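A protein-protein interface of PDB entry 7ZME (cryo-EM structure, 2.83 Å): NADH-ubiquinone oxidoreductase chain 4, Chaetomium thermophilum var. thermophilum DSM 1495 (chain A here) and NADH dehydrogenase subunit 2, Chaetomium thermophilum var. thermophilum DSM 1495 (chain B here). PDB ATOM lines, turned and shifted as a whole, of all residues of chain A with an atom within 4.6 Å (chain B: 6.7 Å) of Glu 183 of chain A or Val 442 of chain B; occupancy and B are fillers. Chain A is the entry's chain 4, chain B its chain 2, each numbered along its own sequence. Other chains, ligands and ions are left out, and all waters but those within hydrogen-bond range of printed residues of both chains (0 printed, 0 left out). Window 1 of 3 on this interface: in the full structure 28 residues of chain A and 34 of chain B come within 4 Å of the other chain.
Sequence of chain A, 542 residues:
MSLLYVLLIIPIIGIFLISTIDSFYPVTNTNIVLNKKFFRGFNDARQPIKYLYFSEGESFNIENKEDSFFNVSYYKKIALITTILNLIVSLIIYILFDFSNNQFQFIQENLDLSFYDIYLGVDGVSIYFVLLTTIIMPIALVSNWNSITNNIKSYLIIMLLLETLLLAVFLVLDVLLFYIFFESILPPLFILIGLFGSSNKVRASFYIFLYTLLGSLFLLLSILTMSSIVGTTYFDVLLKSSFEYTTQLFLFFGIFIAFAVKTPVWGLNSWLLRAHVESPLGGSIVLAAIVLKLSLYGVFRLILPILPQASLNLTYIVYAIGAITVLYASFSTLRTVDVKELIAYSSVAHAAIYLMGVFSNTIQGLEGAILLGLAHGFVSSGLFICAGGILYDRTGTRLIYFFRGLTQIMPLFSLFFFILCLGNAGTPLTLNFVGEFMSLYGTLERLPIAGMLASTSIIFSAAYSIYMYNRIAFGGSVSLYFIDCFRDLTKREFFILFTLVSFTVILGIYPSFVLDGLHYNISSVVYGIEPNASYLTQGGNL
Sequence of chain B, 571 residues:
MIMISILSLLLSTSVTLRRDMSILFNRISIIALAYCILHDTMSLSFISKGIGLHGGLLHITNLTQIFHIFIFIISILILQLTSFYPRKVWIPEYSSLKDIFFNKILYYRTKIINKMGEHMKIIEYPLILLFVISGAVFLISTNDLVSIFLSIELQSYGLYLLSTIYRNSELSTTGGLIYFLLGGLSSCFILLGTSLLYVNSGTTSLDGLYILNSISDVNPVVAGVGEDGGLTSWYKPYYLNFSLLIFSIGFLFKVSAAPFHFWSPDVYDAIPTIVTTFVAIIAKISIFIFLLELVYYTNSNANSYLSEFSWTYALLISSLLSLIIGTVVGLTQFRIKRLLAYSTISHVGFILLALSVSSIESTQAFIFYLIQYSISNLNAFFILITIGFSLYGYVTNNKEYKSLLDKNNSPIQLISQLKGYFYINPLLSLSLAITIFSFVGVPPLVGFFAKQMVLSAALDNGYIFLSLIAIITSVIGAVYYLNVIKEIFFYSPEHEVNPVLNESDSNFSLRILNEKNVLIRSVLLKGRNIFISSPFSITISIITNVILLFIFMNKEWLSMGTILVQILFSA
The side-chain hydroxyl (OG) of Ser 184 of chain A lies within hydrogen-bond range of the backbone carbonyl oxygen (O) of Phe 181 of chain A (2.9 Å). The backbone carbonyl oxygen (O) of Phe 437 of chain B sits at hydrogen-bond distance from the backbone NH (N) of Val 442 of chain B (3.3 Å). The side-chain hydroxyl (OH) of Tyr 179 of chain A sits at hydrogen-bond distance from the side-chain hydroxyl (OG) of Ser 216 of chain A, at 3.1 Å.
Tyr 179 of chain A touches Phe 448 of chain B. Pro 443 of chain B touches Ile 180 of chain A. Ile 180 of chain A touches Phe 449 of chain B. Glu 183 of chain A touches Val 442 of chain B (O to CG1, 3.5 Å). Glu 183 of chain A touches Pro 443 of chain B (CB to CD, 3.7 Å). Ser 184 of chain A touches Pro 443 of chain B. Phe 437 of chain B touches Pro 187 of chain A (CE2 to CB, 3.5 Å). Val 442 of chain B touches Pro 187 of chain A. Phe 209 of chain A touches Phe 437 of chain B. Phe 209 of chain A touches Val 442 of chain B.
Of chain B, only Val 442 (3.5 Å) and Pro 443 (3.7 Å) come within 4 Å of Glu 183 of chain A. Of chain A, only Glu 183, Pro 187 and Phe 209 come within 4 Å of Val 442 of chain B. Of the printed residues of chain B, Pro 187 of chain A touches Phe 437 and Val 442. Printed residues of chain B within 4 Å of Tyr 179 of chain A: Phe 448 (3.4 Å). Of the printed residues of chain A, Phe 437 of chain B touches Pro 187 and Phe 209. Printed residues of chain A within 4 Å of Pro 444 of chain B: Ile 180 (3.8 Å). Phe 181 of chain A touches none of the printed residues of chain B. Ser 438 of chain B touches none of the printed residues of chain A. The nearest residue of chain B that does not touch Glu 183 of chain A is Pro 444 of chain B (6.4 Å). The nearest printed residue of chain A that does not touch Pro 444 of chain B is Ser 184 of chain A (4.1 Å).
Of the 12 printed residues of chain A, 6 touch a printed residue of chain B. Hydrophobic or aromatic side chains of chain A that line the printed part of chain B: Tyr 179, Ile 180, Pro 187 and Phe 209. Hydrophobic or aromatic side chains of chain B that line the printed part of chain A: Phe 437, Val 442, Pro 443, Pro 444, Phe 448 and Phe 449.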
ATOM      1  N   TYR A 179     -26.870  15.992  14.979  1.00  0.00           N
ATOM      2  CA  TYR A 179     -26.699  16.532  13.635  1.00  0.00           C
ATOM      3  C   TYR A 179     -25.393  17.308  13.509  1.00  0.00           C
ATOM      4  O   TYR A 179     -24.779  17.333  12.437  1.00  0.00           O
ATOM      5  CB  TYR A 179     -27.897  17.416  13.287  1.00  0.00           C
ATOM      6  CG  TYR A 179     -27.813  18.111  11.948  1.00  0.00           C
ATOM      7  CD1 TYR A 179     -27.174  19.334  11.816  1.00  0.00           C
ATOM      8  CD2 TYR A 179     -28.379  17.545  10.817  1.00  0.00           C
ATOM      9  CE1 TYR A 179     -27.092  19.964  10.601  1.00  0.00           C
ATOM     10  CE2 TYR A 179     -28.303  18.174   9.599  1.00  0.00           C
ATOM     11  CZ  TYR A 179     -27.660  19.384   9.497  1.00  0.00           C
ATOM     12  OH  TYR A 179     -27.584  20.015   8.281  1.00  0.00           O
ATOM     13  N   ILE A 180     -24.957  17.954  14.591  1.00  0.00           N
ATOM     14  CA  ILE A 180     -23.756  18.784  14.540  1.00  0.00           C
ATOM     15  C   ILE A 180     -22.531  17.939  14.220  1.00  0.00           C
ATOM     16  O   ILE A 180     -21.634  18.372  13.486  1.00  0.00           O
ATOM     17  CB  ILE A 180     -23.601  19.563  15.859  1.00  0.00           C
ATOM     18  CG1 ILE A 180     -24.558  20.754  15.872  1.00  0.00           C
ATOM     19  CG2 ILE A 180     -22.157  20.002  16.079  1.00  0.00           C
ATOM     20  CD1 ILE A 180     -24.696  21.418  17.210  1.00  0.00           C
ATOM     21  N   PHE A 181     -22.533  16.702  14.687  1.00  0.00           N
ATOM     22  CA  PHE A 181     -21.361  15.827  14.489  1.00  0.00           C
ATOM     23  C   PHE A 181     -21.564  14.911  13.268  1.00  0.00           C
ATOM     24  O   PHE A 181     -20.560  14.490  12.685  1.00  0.00           O
ATOM     25  CB  PHE A 181     -21.047  15.166  15.827  1.00  0.00           C
ATOM     26  CG  PHE A 181     -20.475  16.080  16.877  1.00  0.00           C
ATOM     27  CD1 PHE A 181     -19.174  16.543  16.780  1.00  0.00           C
ATOM     28  CD2 PHE A 181     -21.227  16.457  17.975  1.00  0.00           C
ATOM     29  CE1 PHE A 181     -18.646  17.379  17.750  1.00  0.00           C
ATOM     30  CE2 PHE A 181     -20.700  17.291  18.946  1.00  0.00           C
ATOM     31  CZ  PHE A 181     -19.410  17.750  18.830  1.00  0.00           C
ATOM     32  N   PHE A 182     -22.802  14.599  12.899  1.00  0.00           N
ATOM     33  CA  PHE A 182     -23.126  13.778  11.707  1.00  0.00           C
ATOM     34  C   PHE A 182     -22.632  14.543  10.487  1.00  0.00           C
ATOM     35  O   PHE A 182     -22.175  13.904   9.534  1.00  0.00           O
ATOM     36  CB  PHE A 182     -24.653  13.644  11.649  1.00  0.00           C
ATOM     37  CG  PHE A 182     -25.302  12.625  10.748  1.00  0.00           C
ATOM     38  CD1 PHE A 182     -25.002  11.280  10.842  1.00  0.00           C
ATOM     39  CD2 PHE A 182     -26.312  13.010   9.881  1.00  0.00           C
ATOM     40  CE1 PHE A 182     -25.640  10.359  10.025  1.00  0.00           C
ATOM     41  CE2 PHE A 182     -26.946  12.090   9.063  1.00  0.00           C
ATOM     42  CZ  PHE A 182     -26.612  10.760   9.141  1.00  0.00           C
ATOM     43  N   GLU A 183     -22.779  15.869  10.495  1.00  0.00           N
ATOM     44  CA  GLU A 183     -22.402  16.706   9.334  1.00  0.00           C
ATOM     45  C   GLU A 183     -21.017  17.319   9.510  1.00  0.00           C
ATOM     46  O   GLU A 183     -20.553  17.948   8.553  1.00  0.00           O
ATOM     47  CB  GLU A 183     -23.429  17.811   9.142  1.00  0.00           C
ATOM     48  CG  GLU A 183     -24.604  17.402   8.292  1.00  0.00           C
ATOM     49  CD  GLU A 183     -25.212  16.089   8.739  1.00  0.00           C
ATOM     50  OE1 GLU A 183     -25.810  16.066   9.824  1.00  0.00           O
ATOM     51  OE2 GLU A 183     -25.050  15.088   8.010  1.00  0.00           O
ATOM     52  N   SER A 184     -20.360  17.097  10.643  1.00  0.00           N
ATOM     53  CA  SER A 184     -19.050  17.750  10.880  1.00  0.00           C
ATOM     54  C   SER A 184     -17.960  16.969  10.153  1.00  0.00           C
ATOM     55  O   SER A 184     -16.907  17.555   9.894  1.00  0.00           O
ATOM     56  CB  SER A 184     -18.736  17.793  12.349  1.00  0.00           C
ATOM     57  OG  SER A 184     -18.437  16.495  12.834  1.00  0.00           O
ATOM     58  N   ILE A 185     -18.207  15.700   9.851  1.00  0.00           N
ATOM     59  CA  ILE A 185     -17.237  14.858   9.154  1.00  0.00           C
ATOM     60  C   ILE A 185     -17.080  15.211   7.684  1.00  0.00           C
ATOM     61  O   ILE A 185     -16.180  14.679   7.026  1.00  0.00           O
ATOM     62  CB  ILE A 185     -17.636  13.376   9.275  1.00  0.00           C
ATOM     63  CG1 ILE A 185     -19.031  13.160   8.679  1.00  0.00           C
ATOM     64  CG2 ILE A 185     -17.584  12.924  10.729  1.00  0.00           C
ATOM     65  CD1 ILE A 185     -19.338  11.726   8.339  1.00  0.00           C
ATOM     66  N   LEU A 186     -17.938  16.086   7.150  1.00  0.00           N
ATOM     67  CA  LEU A 186     -17.880  16.394   5.722  1.00  0.00           C
ATOM     68  C   LEU A 186     -16.584  17.082   5.310  1.00  0.00           C
ATOM     69  O   LEU A 186     -16.005  16.686   4.283  1.00  0.00           O
ATOM     70  CB  LEU A 186     -19.109  17.211   5.316  1.00  0.00           C
ATOM     71  CG  LEU A 186     -20.222  16.407   4.650  1.00  0.00           C
ATOM     72  CD1 LEU A 186     -20.574  15.237   5.543  1.00  0.00           C
ATOM     73  CD2 LEU A 186     -21.435  17.274   4.370  1.00  0.00           C
ATOM     74  N   PRO A 187     -16.086  18.103   6.009  1.00  0.00           N
ATOM     75  CA  PRO A 187     -14.833  18.741   5.582  1.00  0.00           C
ATOM     76  C   PRO A 187     -13.638  17.803   5.659  1.00  0.00           C
ATOM     77  O   PRO A 187     -12.870  17.728   4.691  1.00  0.00           O
ATOM     78  CB  PRO A 187     -14.701  19.930   6.546  1.00  0.00           C
ATOM     79  CG  PRO A 187     -16.103  20.281   6.830  1.00  0.00           C
ATOM     80  CD  PRO A 187     -16.778  18.948   6.999  1.00  0.00           C
ATOM     81  N   PHE A 209     -19.938  15.159  -0.509  1.00  0.00           N
ATOM     82  CA  PHE A 209     -20.268  16.363   0.287  1.00  0.00           C
ATOM     83  C   PHE A 209     -21.660  16.860  -0.097  1.00  0.00           C
ATOM     84  O   PHE A 209     -22.440  17.157   0.798  1.00  0.00           O
ATOM     85  CB  PHE A 209     -19.167  17.422   0.130  1.00  0.00           C
ATOM     86  CG  PHE A 209     -19.258  18.609   1.056  1.00  0.00           C
ATOM     87  CD1 PHE A 209     -20.201  19.604   0.858  1.00  0.00           C
ATOM     88  CD2 PHE A 209     -18.378  18.746   2.115  1.00  0.00           C
ATOM     89  CE1 PHE A 209     -20.280  20.693   1.709  1.00  0.00           C
ATOM     90  CE2 PHE A 209     -18.456  19.836   2.968  1.00  0.00           C
ATOM     91  CZ  PHE A 209     -19.407  20.806   2.763  1.00  0.00           C
ATOM     92  N   THR A 212     -24.676  14.372   0.973  1.00  0.00           N
ATOM     93  CA  THR A 212     -24.776  14.452   2.448  1.00  0.00           C
ATOM     94  C   THR A 212     -25.272  15.840   2.832  1.00  0.00           C
ATOM     95  O   THR A 212     -26.165  15.891   3.675  1.00  0.00           O
ATOM     96  CB  THR A 212     -23.449  14.138   3.143  1.00  0.00           C
ATOM     97  OG1 THR A 212     -22.841  13.026   2.493  1.00  0.00           O
ATOM     98  CG2 THR A 212     -23.625  13.837   4.612  1.00  0.00           C
ATOM     99  N   SER A 216     -28.993  16.053   4.590  1.00  0.00           N
ATOM    100  CA  SER A 216     -28.939  16.539   5.987  1.00  0.00           C
ATOM    101  C   SER A 216     -29.806  17.785   6.171  1.00  0.00           C
ATOM    102  O   SER A 216     -30.400  17.906   7.238  1.00  0.00           O
ATOM    103  CB  SER A 216     -27.530  16.810   6.376  1.00  0.00           C
ATOM    104  OG  SER A 216     -27.102  18.069   5.884  1.00  0.00           O
ATOM    105  N   ILE B 436     -14.381  29.385   4.520  1.00  0.00           N
ATOM    106  CA  ILE B 436     -15.264  28.999   3.423  1.00  0.00           C
ATOM    107  C   ILE B 436     -16.290  27.978   3.890  1.00  0.00           C
ATOM    108  O   ILE B 436     -17.474  28.072   3.546  1.00  0.00           O
ATOM    109  CB  ILE B 436     -14.443  28.481   2.229  1.00  0.00           C
ATOM    110  CG1 ILE B 436     -13.515  29.574   1.705  1.00  0.00           C
ATOM    111  CG2 ILE B 436     -15.344  27.977   1.131  1.00  0.00           C
ATOM    112  CD1 ILE B 436     -14.250  30.806   1.227  1.00  0.00           C
ATOM    113  N   PHE B 437     -15.861  26.984   4.671  1.00  0.00           N
ATOM    114  CA  PHE B 437     -16.806  26.000   5.187  1.00  0.00           C
ATOM    115  C   PHE B 437     -17.827  26.645   6.111  1.00  0.00           C
ATOM    116  O   PHE B 437     -18.945  26.137   6.254  1.00  0.00           O
ATOM    117  CB  PHE B 437     -16.058  24.878   5.910  1.00  0.00           C
ATOM    118  CG  PHE B 437     -15.519  23.821   4.993  1.00  0.00           C
ATOM    119  CD1 PHE B 437     -16.301  23.298   3.982  1.00  0.00           C
ATOM    120  CD2 PHE B 437     -14.226  23.357   5.134  1.00  0.00           C
ATOM    121  CE1 PHE B 437     -15.805  22.331   3.136  1.00  0.00           C
ATOM    122  CE2 PHE B 437     -13.724  22.394   4.286  1.00  0.00           C
ATOM    123  CZ  PHE B 437     -14.516  21.878   3.290  1.00  0.00           C
ATOM    124  N   SER B 438     -17.465  27.762   6.743  1.00  0.00           N
ATOM    125  CA  SER B 438     -18.413  28.497   7.569  1.00  0.00           C
ATOM    126  C   SER B 438     -19.415  29.263   6.716  1.00  0.00           C
ATOM    127  O   SER B 438     -20.552  29.479   7.143  1.00  0.00           O
ATOM    128  CB  SER B 438     -17.657  29.438   8.505  1.00  0.00           C
ATOM    129  OG  SER B 438     -18.517  30.048   9.447  1.00  0.00           O
ATOM    130  N   PHE B 439     -19.017  29.681   5.514  1.00  0.00           N
ATOM    131  CA  PHE B 439     -19.967  30.248   4.567  1.00  0.00           C
ATOM    132  C   PHE B 439     -20.928  29.207   4.019  1.00  0.00           C
ATOM    133  O   PHE B 439     -22.070  29.549   3.696  1.00  0.00           O
ATOM    134  CB  PHE B 439     -19.242  30.917   3.399  1.00  0.00           C
ATOM    135  CG  PHE B 439     -18.472  32.143   3.776  1.00  0.00           C
ATOM    136  CD1 PHE B 439     -18.888  32.945   4.820  1.00  0.00           C
ATOM    137  CD2 PHE B 439     -17.336  32.502   3.072  1.00  0.00           C
ATOM    138  CE1 PHE B 439     -18.176  34.077   5.163  1.00  0.00           C
ATOM    139  CE2 PHE B 439     -16.622  33.629   3.408  1.00  0.00           C
ATOM    140  CZ  PHE B 439     -17.041  34.419   4.453  1.00  0.00           C
ATOM    141  N   VAL B 440     -20.489  27.955   3.884  1.00  0.00           N
ATOM    142  CA  VAL B 440     -21.396  26.889   3.473  1.00  0.00           C
ATOM    143  C   VAL B 440     -22.459  26.656   4.537  1.00  0.00           C
ATOM    144  O   VAL B 440     -23.648  26.522   4.227  1.00  0.00           O
ATOM    145  CB  VAL B 440     -20.609  25.599   3.169  1.00  0.00           C
ATOM    146  CG1 VAL B 440     -21.557  24.453   2.885  1.00  0.00           C
ATOM    147  CG2 VAL B 440     -19.677  25.809   2.005  1.00  0.00           C
ATOM    148  N   GLY B 441     -22.055  26.623   5.802  1.00  0.00           N
ATOM    149  CA  GLY B 441     -22.975  26.335   6.883  1.00  0.00           C
ATOM    150  C   GLY B 441     -22.779  24.949   7.453  1.00  0.00           C
ATOM    151  O   GLY B 441     -23.748  24.247   7.751  1.00  0.00           O
ATOM    152  N   VAL B 442     -21.526  24.551   7.609  1.00  0.00           N
ATOM    153  CA  VAL B 442     -21.156  23.208   8.047  1.00  0.00           C
ATOM    154  C   VAL B 442     -20.894  23.247   9.547  1.00  0.00           C
ATOM    155  O   VAL B 442     -20.135  24.110  10.004  1.00  0.00           O
ATOM    156  CB  VAL B 442     -19.914  22.698   7.293  1.00  0.00           C
ATOM    157  CG1 VAL B 442     -19.682  21.225   7.563  1.00  0.00           C
ATOM    158  CG2 VAL B 442     -20.059  22.956   5.810  1.00  0.00           C
ATOM    159  N   PRO B 443     -21.475  22.347  10.332  1.00  0.00           N
ATOM    160  CA  PRO B 443     -21.198  22.327  11.767  1.00  0.00           C
ATOM    161  C   PRO B 443     -19.791  21.823  12.035  1.00  0.00           C
ATOM    162  O   PRO B 443     -19.219  21.098  11.209  1.00  0.00           O
ATOM    163  CB  PRO B 443     -22.256  21.359  12.326  1.00  0.00           C
ATOM    164  CG  PRO B 443     -23.142  20.996  11.178  1.00  0.00           C
ATOM    165  CD  PRO B 443     -22.391  21.268   9.931  1.00  0.00           C
ATOM    166  N   PRO B 444     -19.193  22.180  13.182  1.00  0.00           N
ATOM    167  CA  PRO B 444     -19.747  23.027  14.237  1.00  0.00           C
ATOM    168  C   PRO B 444     -19.268  24.471  14.146  1.00  0.00           C
ATOM    169  O   PRO B 444     -18.981  25.086  15.171  1.00  0.00           O
ATOM    170  CB  PRO B 444     -19.217  22.361  15.499  1.00  0.00           C
ATOM    171  CG  PRO B 444     -17.854  21.915  15.090  1.00  0.00           C
ATOM    172  CD  PRO B 444     -17.922  21.575  13.611  1.00  0.00           C
ATOM    173  N   LEU B 445     -19.182  24.995  12.929  1.00  0.00           N
ATOM    174  CA  LEU B 445     -18.670  26.338  12.716  1.00  0.00           C
ATOM    175  C   LEU B 445     -19.758  27.372  12.975  1.00  0.00           C
ATOM    176  O   LEU B 445     -20.952  27.070  13.012  1.00  0.00           O
ATOM    177  CB  LEU B 445     -18.112  26.473  11.301  1.00  0.00           C
ATOM    178  CG  LEU B 445     -17.097  25.391  10.937  1.00  0.00           C
ATOM    179  CD1 LEU B 445     -16.537  25.612   9.545  1.00  0.00           C
ATOM    180  CD2 LEU B 445     -15.985  25.328  11.970  1.00  0.00           C
ATOM    181  N   VAL B 446     -19.326  28.621  13.161  1.00  0.00           N
ATOM    182  CA  VAL B 446     -20.255  29.683  13.529  1.00  0.00           C
ATOM    183  C   VAL B 446     -21.263  29.949  12.415  1.00  0.00           C
ATOM    184  O   VAL B 446     -22.394  30.367  12.682  1.00  0.00           O
ATOM    185  CB  VAL B 446     -19.466  30.951  13.924  1.00  0.00           C
ATOM    186  CG1 VAL B 446     -18.715  31.528  12.734  1.00  0.00           C
ATOM    187  CG2 VAL B 446     -20.381  31.980  14.554  1.00  0.00           C
ATOM    188  N   GLY B 447     -20.888  29.702  11.159  1.00  0.00           N
ATOM    189  CA  GLY B 447     -21.803  29.953  10.060  1.00  0.00           C
ATOM    190  C   GLY B 447     -22.952  28.969   9.991  1.00  0.00           C
ATOM    191  O   GLY B 447     -24.034  29.312   9.508  1.00  0.00           O
ATOM    192  N   PHE B 448     -22.739  27.738  10.457  1.00  0.00           N
ATOM    193  CA  PHE B 448     -23.845  26.795  10.562  1.00  0.00           C
ATOM    194  C   PHE B 448     -24.889  27.271  11.559  1.00  0.00           C
ATOM    195  O   PHE B 448     -26.089  27.225  11.276  1.00  0.00           O
ATOM    196  CB  PHE B 448     -23.340  25.416  10.981  1.00  0.00           C
ATOM    197  CG  PHE B 448     -24.411  24.550  11.572  1.00  0.00           C
ATOM    198  CD1 PHE B 448     -25.368  23.966  10.764  1.00  0.00           C
ATOM    199  CD2 PHE B 448     -24.488  24.358  12.944  1.00  0.00           C
ATOM    200  CE1 PHE B 448     -26.366  23.196  11.308  1.00  0.00           C
ATOM    201  CE2 PHE B 448     -25.486  23.588  13.488  1.00  0.00           C
ATOM    202  CZ  PHE B 448     -26.425  23.003  12.670  1.00  0.00           C
ATOM    203  N   PHE B 449     -24.443  27.713  12.733  1.00  0.00           N
ATOM    204  CA  PHE B 449     -25.369  28.134  13.775  1.00  0.00           C
ATOM    205  C   PHE B 449     -26.130  29.379  13.358  1.00  0.00           C
ATOM    206  O   PHE B 449     -27.309  29.536  13.692  1.00  0.00           O
ATOM    207  CB  PHE B 449     -24.605  28.371  15.074  1.00  0.00           C
ATOM    208  CG  PHE B 449     -24.131  27.114  15.726  1.00  0.00           C
ATOM    209  CD1 PHE B 449     -25.008  26.311  16.425  1.00  0.00           C
ATOM    210  CD2 PHE B 449     -22.809  26.723  15.626  1.00  0.00           C
ATOM    211  CE1 PHE B 449     -24.573  25.152  17.022  1.00  0.00           C
ATOM    212  CE2 PHE B 449     -22.372  25.565  16.221  1.00  0.00           C
ATOM    213  CZ  PHE B 449     -23.254  24.779  16.919  1.00  0.00           C
